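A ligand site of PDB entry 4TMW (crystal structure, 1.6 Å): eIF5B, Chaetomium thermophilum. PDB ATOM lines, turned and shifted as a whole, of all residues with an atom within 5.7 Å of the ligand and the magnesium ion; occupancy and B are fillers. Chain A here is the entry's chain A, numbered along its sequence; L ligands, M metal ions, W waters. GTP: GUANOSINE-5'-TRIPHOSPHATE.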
ATOM      1  N   GLY A  17      21.166  25.289  20.741  1.00  0.00           N
ATOM      2  CA  GLY A  17      20.255  24.510  21.551  1.00  0.00           C
ATOM      3  C   GLY A  17      19.840  23.256  20.792  1.00  0.00           C
ATOM      4  O   GLY A  17      20.028  23.180  19.572  1.00  0.00           O
ATOM      5  N   HIS A  18      19.189  22.350  21.505  1.00  0.00           N
ATOM      6  CA  HIS A  18      18.729  21.101  20.931  1.00  0.00           C
ATOM      7  C   HIS A  18      17.616  21.384  19.930  1.00  0.00           C
ATOM      8  O   HIS A  18      17.065  22.464  19.925  1.00  0.00           O
ATOM      9  CB  HIS A  18      18.227  20.194  22.063  1.00  0.00           C
ATOM     10  CG  HIS A  18      17.932  18.786  21.626  1.00  0.00           C
ATOM     11  ND1 HIS A  18      18.899  17.823  21.521  1.00  0.00           N
ATOM     12  CD2 HIS A  18      16.767  18.197  21.296  1.00  0.00           C
ATOM     13  CE1 HIS A  18      18.352  16.689  21.123  1.00  0.00           C
ATOM     14  NE2 HIS A  18      17.056  16.888  20.981  1.00  0.00           N
ATOM     15  N   VAL A  19      17.337  20.425  19.057  1.00  0.00           N
ATOM     16  CA  VAL A  19      16.364  20.665  17.998  1.00  0.00           C
ATOM     17  C   VAL A  19      14.996  21.034  18.578  1.00  0.00           C
ATOM     18  O   VAL A  19      14.577  20.505  19.591  1.00  0.00           O
ATOM     19  CB  VAL A  19      16.212  19.442  17.076  1.00  0.00           C
ATOM     20  CG1 VAL A  19      15.504  18.300  17.811  1.00  0.00           C
ATOM     21  CG2 VAL A  19      15.459  19.805  15.812  1.00  0.00           C
ATOM     22  N   ASP A  20      14.349  21.993  17.940  1.00  0.00           N
ATOM     23  CA  ASP A  20      12.978  22.397  18.245  1.00  0.00           C
ATOM     24  C   ASP A  20      12.786  23.016  19.637  1.00  0.00           C
ATOM     25  O   ASP A  20      11.687  23.015  20.172  1.00  0.00           O
ATOM     26  CB  ASP A  20      12.023  21.222  18.064  1.00  0.00           C
ATOM     27  CG  ASP A  20      11.693  20.951  16.601  1.00  0.00           C
ATOM     28  OD1 ASP A  20      11.952  21.829  15.762  1.00  0.00           O
ATOM     29  OD2 ASP A  20      11.186  19.858  16.300  1.00  0.00           O
ATOM     30  N   THR A  21      13.849  23.574  20.193  1.00  0.00           N
ATOM     31  CA  THR A  21      13.743  24.186  21.506  1.00  0.00           C
ATOM     32  C   THR A  21      13.200  25.618  21.433  1.00  0.00           C
ATOM     33  O   THR A  21      12.866  26.191  22.451  1.00  0.00           O
ATOM     34  CB  THR A  21      15.080  24.161  22.275  1.00  0.00           C
ATOM     35  OG1 THR A  21      16.139  24.592  21.423  1.00  0.00           O
ATOM     36  CG2 THR A  21      15.367  22.755  22.768  1.00  0.00           C
ATOM     37  N   GLY A  22      13.063  26.152  20.223  1.00  0.00           N
ATOM     38  CA  GLY A  22      12.578  27.505  20.043  1.00  0.00           C
ATOM     39  C   GLY A  22      13.549  28.613  19.671  1.00  0.00           C
ATOM     40  O   GLY A  22      13.211  29.786  19.792  1.00  0.00           O
ATOM     41  N   LYS A  23      14.757  28.268  19.227  1.00  0.00           N
ATOM     42  CA  LYS A  23      15.718  29.302  18.899  1.00  0.00           C
ATOM     43  C   LYS A  23      15.229  30.240  17.800  1.00  0.00           C
ATOM     44  O   LYS A  23      15.238  31.450  17.965  1.00  0.00           O
ATOM     45  CB  LYS A  23      17.003  28.643  18.391  1.00  0.00           C
ATOM     46  CG  LYS A  23      17.547  27.526  19.265  1.00  0.00           C
ATOM     47  CD  LYS A  23      18.778  26.877  18.624  1.00  0.00           C
ATOM     48  CE  LYS A  23      18.398  25.866  17.555  1.00  0.00           C
ATOM     49  NZ  LYS A  23      17.793  24.629  18.131  1.00  0.00           N
ATOM     50  N   THR A  24      14.744  29.683  16.698  1.00  0.00           N
ATOM     51  CA  THR A  24      14.210  30.498  15.613  1.00  0.00           C
ATOM     52  C   THR A  24      12.928  31.218  16.008  1.00  0.00           C
ATOM     53  O   THR A  24      12.725  32.369  15.678  1.00  0.00           O
ATOM     54  CB  THR A  24      14.003  29.690  14.328  1.00  0.00           C
ATOM     55  OG1 THR A  24      15.245  29.107  13.941  1.00  0.00           O
ATOM     56  CG2 THR A  24      13.511  30.581  13.210  1.00  0.00           C
ATOM     57  N   LYS A  25      12.060  30.500  16.721  1.00  0.00           N
ATOM     58  CA  LYS A  25      10.802  31.157  17.168  1.00  0.00           C
ATOM     59  C   LYS A  25      11.063  32.370  18.074  1.00  0.00           C
ATOM     60  O   LYS A  25      10.368  33.414  17.968  1.00  0.00           O
ATOM     61  CB  LYS A  25       9.933  30.110  17.916  1.00  0.00           C
ATOM     62  CG  LYS A  25       8.408  30.435  17.869  1.00  0.00           C
ATOM     63  CD  LYS A  25       7.875  30.146  16.431  1.00  0.00           C
ATOM     64  CE  LYS A  25       6.375  30.345  16.304  1.00  0.00           C
ATOM     65  NZ  LYS A  25       6.095  30.064  14.874  1.00  0.00           N
ATOM     66  N   LEU A  26      12.063  32.281  18.934  1.00  0.00           N
ATOM     67  CA  LEU A  26      12.453  33.462  19.767  1.00  0.00           C
ATOM     68  C   LEU A  26      12.873  34.613  18.901  1.00  0.00           C
ATOM     69  O   LEU A  26      12.406  35.734  19.111  1.00  0.00           O
ATOM     70  CB  LEU A  26      13.580  33.099  20.725  1.00  0.00           C
ATOM     71  CG  LEU A  26      13.212  32.277  21.963  1.00  0.00           C
ATOM     72  CD1 LEU A  26      14.469  31.639  22.642  1.00  0.00           C
ATOM     73  CD2 LEU A  26      12.487  33.159  22.999  1.00  0.00           C
ATOM     74  N   GLN A  36      10.265  30.685  10.859  1.00  0.00           N
ATOM     75  CA  GLN A  36      10.109  29.296  11.243  1.00  0.00           C
ATOM     76  C   GLN A  36       8.983  28.630  10.453  1.00  0.00           C
ATOM     77  O   GLN A  36       9.099  27.428  10.093  1.00  0.00           O
ATOM     78  CB  GLN A  36       9.848  29.186  12.768  1.00  0.00           C
ATOM     79  CG  GLN A  36      10.112  27.791  13.319  1.00  0.00           C
ATOM     80  CD  GLN A  36       8.894  26.874  13.232  1.00  0.00           C
ATOM     81  OE1 GLN A  36       7.711  27.343  13.070  1.00  0.00           O
ATOM     82  NE2 GLN A  36       9.143  25.567  13.290  1.00  0.00           N
ATOM     83  N   GLU A  39      10.214  27.306   7.112  1.00  0.00           N
ATOM     84  CA  GLU A  39      11.267  26.305   7.070  1.00  0.00           C
ATOM     85  C   GLU A  39      10.765  24.922   6.701  1.00  0.00           C
ATOM     86  O   GLU A  39       9.745  24.485   7.210  1.00  0.00           O
ATOM     87  CB  GLU A  39      11.962  26.224   8.432  1.00  0.00           C
ATOM     88  CG  GLU A  39      12.872  27.390   8.735  1.00  0.00           C
ATOM     89  CD  GLU A  39      13.500  27.270  10.104  1.00  0.00           C
ATOM     90  OE1 GLU A  39      12.899  26.609  10.967  1.00  0.00           O
ATOM     91  OE2 GLU A  39      14.591  27.833  10.302  1.00  0.00           O
ATOM     92  N   GLY A  42      10.026  22.514   9.498  1.00  0.00           N
ATOM     93  CA  GLY A  42      10.085  23.380  10.658  1.00  0.00           C
ATOM     94  C   GLY A  42      11.442  23.316  11.339  1.00  0.00           C
ATOM     95  O   GLY A  42      11.543  23.563  12.526  1.00  0.00           O
ATOM     96  N   ILE A  43      12.492  23.022  10.583  1.00  0.00           N
ATOM     97  CA  ILE A  43      13.834  22.969  11.148  1.00  0.00           C
ATOM     98  C   ILE A  43      14.802  23.875  10.416  1.00  0.00           C
ATOM     99  O   ILE A  43      14.728  24.050   9.211  1.00  0.00           O
ATOM    100  CB  ILE A  43      14.414  21.537  11.181  1.00  0.00           C
ATOM    101  CG1 ILE A  43      14.414  20.911   9.788  1.00  0.00           C
ATOM    102  CG2 ILE A  43      13.686  20.662  12.192  1.00  0.00           C
ATOM    103  CD1 ILE A  43      15.336  19.725   9.680  1.00  0.00           C
ATOM    104  N   THR A  44      15.732  24.462  11.169  1.00  0.00           N
ATOM    105  CA  THR A  44      16.766  25.308  10.609  1.00  0.00           C
ATOM    106  C   THR A  44      17.888  24.439  10.022  1.00  0.00           C
ATOM    107  O   THR A  44      18.352  23.516  10.671  1.00  0.00           O
ATOM    108  CB  THR A  44      17.323  26.244  11.681  1.00  0.00           C
ATOM    109  OG1 THR A  44      16.264  27.069  12.177  1.00  0.00           O
ATOM    110  CG2 THR A  44      18.424  27.129  11.114  1.00  0.00           C
ATOM    111  N   ASP A  81      21.765  32.614  14.113  1.00  0.00           N
ATOM    112  CA  ASP A  81      20.878  31.478  14.402  1.00  0.00           C
ATOM    113  C   ASP A  81      21.565  30.225  13.868  1.00  0.00           C
ATOM    114  O   ASP A  81      22.235  30.294  12.815  1.00  0.00           O
ATOM    115  CB  ASP A  81      19.522  31.731  13.692  1.00  0.00           C
ATOM    116  CG  ASP A  81      18.376  30.793  14.194  1.00  0.00           C
ATOM    117  OD1 ASP A  81      18.637  30.046  15.143  1.00  0.00           O
ATOM    118  OD2 ASP A  81      17.255  30.834  13.594  1.00  0.00           O
ATOM    119  N   THR A  82      21.427  29.114  14.595  1.00  0.00           N
ATOM    120  CA  THR A  82      22.030  27.831  14.134  1.00  0.00           C
ATOM    121  C   THR A  82      21.047  26.641  14.176  1.00  0.00           C
ATOM    122  O   THR A  82      20.093  26.686  14.947  1.00  0.00           O
ATOM    123  CB  THR A  82      23.263  27.414  15.026  1.00  0.00           C
ATOM    124  OG1 THR A  82      22.836  27.238  16.378  1.00  0.00           O
ATOM    125  CG2 THR A  82      24.340  28.509  15.000  1.00  0.00           C
ATOM    126  N   PRO A  83      21.248  25.608  13.361  1.00  0.00           N
ATOM    127  CA  PRO A  83      20.405  24.405  13.470  1.00  0.00           C
ATOM    128  C   PRO A  83      20.602  23.656  14.788  1.00  0.00           C
ATOM    129  O   PRO A  83      21.743  23.533  15.293  1.00  0.00           O
ATOM    130  CB  PRO A  83      20.937  23.477  12.355  1.00  0.00           C
ATOM    131  CG  PRO A  83      21.633  24.447  11.379  1.00  0.00           C
ATOM    132  CD  PRO A  83      22.260  25.484  12.287  1.00  0.00           C
ATOM    133  N   GLY A  84      19.516  23.103  15.304  1.00  0.00           N
ATOM    134  CA  GLY A  84      19.671  22.162  16.381  1.00  0.00           C
ATOM    135  C   GLY A  84      19.689  20.703  15.935  1.00  0.00           C
ATOM    136  O   GLY A  84      20.076  19.864  16.728  1.00  0.00           O
ATOM    137  N   HIS A  85      19.175  20.379  14.755  1.00  0.00           N
ATOM    138  CA  HIS A  85      19.127  18.964  14.344  1.00  0.00           C
ATOM    139  C   HIS A  85      20.523  18.349  14.396  1.00  0.00           C
ATOM    140  O   HIS A  85      21.534  18.991  14.051  1.00  0.00           O
ATOM    141  CB  HIS A  85      18.547  18.871  12.932  1.00  0.00           C
ATOM    142  CG  HIS A  85      18.307  17.472  12.480  1.00  0.00           C
ATOM    143  ND1 HIS A  85      19.316  16.676  11.984  1.00  0.00           N
ATOM    144  CD2 HIS A  85      17.183  16.720  12.452  1.00  0.00           C
ATOM    145  CE1 HIS A  85      18.811  15.487  11.650  1.00  0.00           C
ATOM    146  NE2 HIS A  85      17.524  15.493  11.914  1.00  0.00           N
ATOM    147  N   ASN A 135      13.093  28.112  27.805  1.00  0.00           N
ATOM    148  CA  ASN A 135      11.975  28.472  26.941  1.00  0.00           C
ATOM    149  C   ASN A 135      10.737  27.561  27.086  1.00  0.00           C
ATOM    150  O   ASN A 135      10.781  26.451  27.628  1.00  0.00           O
ATOM    151  CB  ASN A 135      12.506  28.529  25.470  1.00  0.00           C
ATOM    152  CG  ASN A 135      11.549  29.189  24.510  1.00  0.00           C
ATOM    153  OD1 ASN A 135      10.923  30.224  24.804  1.00  0.00           O
ATOM    154  ND2 ASN A 135      11.356  28.532  23.339  1.00  0.00           N
ATOM    155  N   LYS A 136       9.615  28.063  26.550  1.00  0.00           N
ATOM    156  CA  LYS A 136       8.300  27.368  26.517  1.00  0.00           C
ATOM    157  C   LYS A 136       7.614  27.408  27.877  1.00  0.00           C
ATOM    158  O   LYS A 136       6.859  26.484  28.206  1.00  0.00           O
ATOM    159  CB  LYS A 136       8.385  25.916  25.969  1.00  0.00           C
ATOM    160  CG  LYS A 136       9.221  25.892  24.627  1.00  0.00           C
ATOM    161  CD  LYS A 136       8.801  24.669  23.805  1.00  0.00           C
ATOM    162  CE  LYS A 136       9.682  24.558  22.533  1.00  0.00           C
ATOM    163  NZ  LYS A 136       9.292  23.250  21.768  1.00  0.00           N
ATOM    164  N   ILE A 137       7.790  28.508  28.632  1.00  0.00           N
ATOM    165  CA  ILE A 137       7.076  28.582  29.908  1.00  0.00           C
ATOM    166  C   ILE A 137       5.558  28.611  29.772  1.00  0.00           C
ATOM    167  O   ILE A 137       4.880  28.321  30.753  1.00  0.00           O
ATOM    168  CB  ILE A 137       7.505  29.806  30.750  1.00  0.00           C
ATOM    169  CG1 ILE A 137       7.193  31.125  30.031  1.00  0.00           C
ATOM    170  CG2 ILE A 137       8.990  29.647  31.125  1.00  0.00           C
ATOM    171  CD1 ILE A 137       7.803  32.397  30.801  1.00  0.00           C
ATOM    172  N   ASP A 138       5.021  28.980  28.585  1.00  0.00           N
ATOM    173  CA  ASP A 138       3.575  28.959  28.436  1.00  0.00           C
ATOM    174  C   ASP A 138       3.012  27.519  28.482  1.00  0.00           C
ATOM    175  O   ASP A 138       1.780  27.321  28.562  1.00  0.00           O
ATOM    176  CB  ASP A 138       3.244  29.633  27.104  1.00  0.00           C
ATOM    177  CG  ASP A 138       3.904  28.874  25.936  1.00  0.00           C
ATOM    178  OD1 ASP A 138       3.197  28.061  25.304  1.00  0.00           O
ATOM    179  OD2 ASP A 138       5.120  29.096  25.744  1.00  0.00           O
ATOM    180  N   ARG A 139       3.897  26.493  28.398  1.00  0.00           N
ATOM    181  CA  ARG A 139       3.480  25.115  28.518  1.00  0.00           C
ATOM    182  C   ARG A 139       3.317  24.667  29.953  1.00  0.00           C
ATOM    183  O   ARG A 139       2.826  23.563  30.202  1.00  0.00           O
ATOM    184  CB  ARG A 139       4.478  24.190  27.773  1.00  0.00           C
ATOM    185  CG  ARG A 139       4.379  24.446  26.265  1.00  0.00           C
ATOM    186  CD  ARG A 139       4.893  23.301  25.461  1.00  0.00           C
ATOM    187  NE  ARG A 139       3.868  22.273  25.382  1.00  0.00           N
ATOM    188  CZ  ARG A 139       3.991  21.036  25.831  1.00  0.00           C
ATOM    189  NH1 ARG A 139       2.963  20.207  25.714  1.00  0.00           N
ATOM    190  NH2 ARG A 139       5.131  20.621  26.392  1.00  0.00           N
ATOM    191  N   THR A 202      11.550  32.094  29.338  1.00  0.00           N
ATOM    192  CA  THR A 202      10.981  32.782  28.165  1.00  0.00           C
ATOM    193  C   THR A 202       9.846  31.992  27.574  1.00  0.00           C
ATOM    194  O   THR A 202       9.734  30.776  27.790  1.00  0.00           O
ATOM    195  CB  THR A 202      12.010  32.954  27.033  1.00  0.00           C
ATOM    196  OG1 THR A 202      12.509  31.693  26.600  1.00  0.00           O
ATOM    197  CG2 THR A 202      13.235  33.747  27.541  1.00  0.00           C
ATOM    198  N   SER A 203       9.009  32.695  26.803  1.00  0.00           N
ATOM    199  CA  SER A 203       8.139  32.042  25.854  1.00  0.00           C
ATOM    200  C   SER A 203       8.276  32.775  24.527  1.00  0.00           C
ATOM    201  O   SER A 203       8.026  33.958  24.449  1.00  0.00           O
ATOM    202  CB  SER A 203       6.668  32.147  26.263  1.00  0.00           C
ATOM    203  OG  SER A 203       5.815  31.654  25.188  1.00  0.00           O
ATOM    204  N   ALA A 204       8.720  32.051  23.497  1.00  0.00           N
ATOM    205  CA  ALA A 204       8.700  32.608  22.148  1.00  0.00           C
ATOM    206  C   ALA A 204       7.313  32.781  21.608  1.00  0.00           C
ATOM    207  O   ALA A 204       7.124  33.575  20.694  1.00  0.00           O
ATOM    208  CB  ALA A 204       9.527  31.669  21.170  1.00  0.00           C
ATOM    209  N   HIS A 205       6.334  32.047  22.127  1.00  0.00           N
ATOM    210  CA  HIS A 205       4.970  32.237  21.654  1.00  0.00           C
ATOM    211  C   HIS A 205       4.323  33.532  22.240  1.00  0.00           C
ATOM    212  O   HIS A 205       3.700  34.299  21.514  1.00  0.00           O
ATOM    213  CB  HIS A 205       4.141  31.011  21.969  1.00  0.00           C
ATOM    214  CG  HIS A 205       4.368  29.879  21.004  1.00  0.00           C
ATOM    215  ND1 HIS A 205       3.515  28.787  20.919  1.00  0.00           N
ATOM    216  CD2 HIS A 205       5.350  29.682  20.085  1.00  0.00           C
ATOM    217  CE1 HIS A 205       3.969  27.980  19.970  1.00  0.00           C
ATOM    218  NE2 HIS A 205       5.041  28.520  19.421  1.00  0.00           N
ATOM    219  N   THR A 206       4.529  33.788  23.538  1.00  0.00           N
ATOM    220  CA  THR A 206       3.872  34.949  24.187  1.00  0.00           C
ATOM    221  C   THR A 206       4.769  36.141  24.255  1.00  0.00           C
ATOM    222  O   THR A 206       4.293  37.279  24.478  1.00  0.00           O
ATOM    223  CB  THR A 206       3.394  34.669  25.623  1.00  0.00           C
ATOM    224  OG1 THR A 206       4.579  34.595  26.461  1.00  0.00           O
ATOM    225  CG2 THR A 206       2.569  33.370  25.727  1.00  0.00           C
ATOM    226  N   ARG A 293      19.717  34.718   5.831  1.00  0.00           N
ATOM    227  CA  ARG A 293      19.480  33.449   5.144  1.00  0.00           C
ATOM    228  C   ARG A 293      18.179  33.452   4.331  1.00  0.00           C
ATOM    229  O   ARG A 293      17.858  32.445   3.661  1.00  0.00           O
ATOM    230  CB  ARG A 293      19.529  32.231   6.125  1.00  0.00           C
ATOM    231  CG  ARG A 293      18.344  32.142   7.084  1.00  0.00           C
ATOM    232  CD  ARG A 293      18.629  31.011   8.060  1.00  0.00           C
ATOM    233  NE  ARG A 293      17.897  31.003   9.282  1.00  0.00           N
ATOM    234  CZ  ARG A 293      16.877  30.196   9.609  1.00  0.00           C
ATOM    235  NH1 ARG A 293      16.313  29.322   8.750  1.00  0.00           N
ATOM    236  NH2 ARG A 293      16.365  30.275  10.798  1.00  0.00           N
HETATM  237  PG  GTP L   1      15.848  23.993  15.090  1.00  0.00           P
HETATM  238  O1G GTP L   1      16.444  25.229  14.494  1.00  0.00           O
HETATM  239  O2G GTP L   1      16.735  23.247  16.038  1.00  0.00           O
HETATM  240  O3G GTP L   1      15.185  23.110  14.084  1.00  0.00           O
HETATM  241  O3B GTP L   1      14.562  24.414  15.977  1.00  0.00           O
HETATM  242  PB  GTP L   1      14.442  25.736  16.901  1.00  0.00           P
HETATM  243  O1B GTP L   1      15.191  25.564  18.187  1.00  0.00           O
HETATM  244  O2B GTP L   1      14.750  26.908  16.043  1.00  0.00           O
HETATM  245  O3A GTP L   1      12.892  25.750  17.307  1.00  0.00           O
HETATM  246  PA  GTP L   1      11.717  26.348  16.396  1.00  0.00           P
HETATM  247  O1A GTP L   1      11.790  25.648  15.075  1.00  0.00           O
HETATM  248  O2A GTP L   1      11.727  27.836  16.442  1.00  0.00           O
HETATM  249  O5' GTP L   1      10.398  25.835  17.146  1.00  0.00           O
HETATM  250  C5' GTP L   1      10.098  24.449  17.226  1.00  0.00           C
HETATM  251  C4' GTP L   1       8.637  24.239  17.601  1.00  0.00           C
HETATM  252  O4' GTP L   1       8.446  24.599  18.963  1.00  0.00           O
HETATM  253  C3' GTP L   1       7.716  25.126  16.788  1.00  0.00           C
HETATM  254  O3' GTP L   1       6.478  24.451  16.584  1.00  0.00           O
HETATM  255  C2' GTP L   1       7.471  26.316  17.693  1.00  0.00           C
HETATM  256  O2' GTP L   1       6.224  26.945  17.421  1.00  0.00           O
HETATM  257  C1' GTP L   1       7.486  25.644  19.058  1.00  0.00           C
HETATM  258  N9  GTP L   1       7.887  26.635  20.071  1.00  0.00           N
HETATM  259  C8  GTP L   1       8.986  27.400  20.070  1.00  0.00           C
HETATM  260  N7  GTP L   1       9.029  28.190  21.159  1.00  0.00           N
HETATM  261  C5  GTP L   1       7.932  27.936  21.872  1.00  0.00           C
HETATM  262  C6  GTP L   1       7.346  28.418  23.137  1.00  0.00           C
HETATM  263  O6  GTP L   1       7.922  29.279  23.816  1.00  0.00           O
HETATM  264  N1  GTP L   1       6.188  27.883  23.527  1.00  0.00           N
HETATM  265  C2  GTP L   1       5.547  26.932  22.828  1.00  0.00           C
HETATM  266  N2  GTP L   1       4.381  26.451  23.296  1.00  0.00           N
HETATM  267  N3  GTP L   1       6.030  26.445  21.663  1.00  0.00           N
HETATM  268  C4  GTP L   1       7.185  26.900  21.158  1.00  0.00           C
HETATM  269 MG    MG M   1      15.685  26.977  14.130  1.00  0.00          MG
HETATM  270  O   HOH W   1       2.678  24.424  21.924  1.00  0.00           O
HETATM  271  O   HOH W   2      17.594  22.137  12.991  1.00  0.00           O
HETATM  272  O   HOH W   3       6.455  23.376  21.483  1.00  0.00           O
HETATM  273  O   HOH W   4      13.762  26.517  13.399  1.00  0.00           O
HETATM  274  O   HOH W   5      17.538  27.681  14.814  1.00  0.00           O
HETATM  275  O   HOH W   6       5.647  22.461  18.971  1.00  0.00           O
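OD2 of Asp 138 sits at hydrogen-bond distance from N1 of the ligand, 2.7 Å away.
ND2 of Asn 135 sits at hydrogen-bond distance from N7 of the ligand (3.2 Å).
The side-chain amide nitrogen of Gln 36 lies within hydrogen-bond range of an oxygen (O1A) of the ligand, 3.2 Å away.
The side-chain amino group (NZ) of Lys 23 is in salt-bridge range of an oxygen (O2G) of the ligand, 2.7 Å away.
NE2 of His 205 is in hydrogen-bond range of O2' of the ligand (2.8 Å).
An oxygen (O2A) of the ligand sits at hydrogen-bond distance from the backbone NH (N) of Lys 25, at 2.7 Å.
O6 of the ligand lies close to OG of Ser 203 (3.5 Å).
O3G of the ligand is in hydrogen-bond range of N of Thr 44.
An oxygen (O1B) of the ligand sits at hydrogen-bond distance from the backbone NH of Thr 21 (3.1 Å).
The side-chain amino group (NZ) of Lys 136 is in hydrogen-bond range of an oxygen (O4') of the ligand, 3.2 Å away.
An oxygen (O2G) of the ligand lies within hydrogen-bond range of the backbone NH (N) of Gly 84 (2.9 Å).
An oxygen (O3B) of the ligand lies within hydrogen-bond range of the backbone NH (N) of Asp 20, 3.1 Å away.
An oxygen (O1B) of the ligand lies within hydrogen-bond range of the backbone NH (N) of Lys 23 (2.9 Å).
The backbone NH (N) of Gly 22 is in hydrogen-bond range of an oxygen (O3A) of the ligand (2.9 Å).
The backbone NH (N) of Lys 136 sits close to an oxygen (O6) of the ligand (3.4 Å).
The backbone NH (N) of Thr 24 sits close to an oxygen (O2B) of the ligand (2.9 Å).
The backbone NH (N) of Ala 204 sits at hydrogen-bond distance from an oxygen (O6) of the ligand.
Water W4 bridges OE1 of Glu 39 (2.6 Å) and O1A of the ligand (2.7 Å).
Water W5 bridges the side-chain carboxylate of Asp 81 and the backbone carbonyl oxygen of Thr 82.
Water W2 lies within hydrogen-bond range of O of Thr 44 (2.8 Å), O3G of the ligand (2.8 Å), N of His 85 (2.9 Å) and N of Gly 84 (3.2 Å).
Water W3 bridges the side-chain amino group (NZ) of Lys 136 and a nitrogen (N3) of the ligand.
The backbone carbonyl oxygen (O) of Asp 20 sits at hydrogen-bond distance from the side-chain amino group (NZ) of Lys 136 (2.9 Å).
OD1 of Asn 135 is in hydrogen-bond range of N of Ala 204, at 3.1 Å.
The backbone NH (N) of Thr 206 sits at hydrogen-bond distance from the side-chain hydroxyl (OG) of Ser 203 (3.0 Å).
The backbone carbonyl oxygen (O) of Gly 42 is in hydrogen-bond range of the side-chain amide nitrogen (NE2) of Gln 36, at 3.2 Å.
The backbone NH (N) of His 205 lies within hydrogen-bond range of the side-chain hydroxyl (OG) of Ser 203, at 3.1 Å.
OG1 of Thr 44 lies close to OE2 of Glu 39.
The side-chain amino group (NZ) of Lys 23 lies within hydrogen-bond range of the backbone carbonyl oxygen (O) of His 18 (2.9 Å).
The side-chain hydroxyl (OG1) of Thr 202 sits at hydrogen-bond distance from the side-chain amide oxygen (OD1) of Asn 135, at 2.8 Å.
The magnesium ion is bound by O1G of the ligand (1.9 Å), OG1 of Thr 44 (2.0 Å), water W5 (2.1 Å), water W4 (2.1 Å), O2B of the ligand (2.1 Å) and OG1 of Thr 24 (2.2 Å).
The magnesium ion has six donor atoms within binding distance.
An oxygen (O1A) of the ligand sits close to the backbone carbonyl oxygen of Gly 42, 3.3 Å away.
His 18 touches the ligand (O to O2G, 3.98 Å).
Val 19 touches the ligand.
Ile 43 touches the ligand (CA to O3G, 3.2 Å).
Thr 82 touches the ligand.
His 85 touches the ligand (N to O2G, 3.98 Å).
CG of Arg 139 touches N2 of the ligand (3.6 Å).
Hydrophobic or aromatic side chains within 4 Å of the ligand: Val 19, Ile 43, Ala 204 and His 205.
22 residues have an atom within 4 Å of the ligand: His 18, Val 19, Asp 20, Thr 21, Gly 22, Lys 23, Thr 24, Lys 25, Gln 36, Gly 42, Ile 43, Thr 44, Thr 82, Gly 84, His 85, Asn 135, Lys 136, Asp 138, Arg 139, Ser 203, Ala 204 and His 205.
Along chain A the residues within 4 Å of the ligand span positions 18 to 205.
The nearest printed residue that does not touch the ligand is Pro 83 (4.1 Å).
Of the 31 residues printed, 2 come within 4 Å of the magnesium ion.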
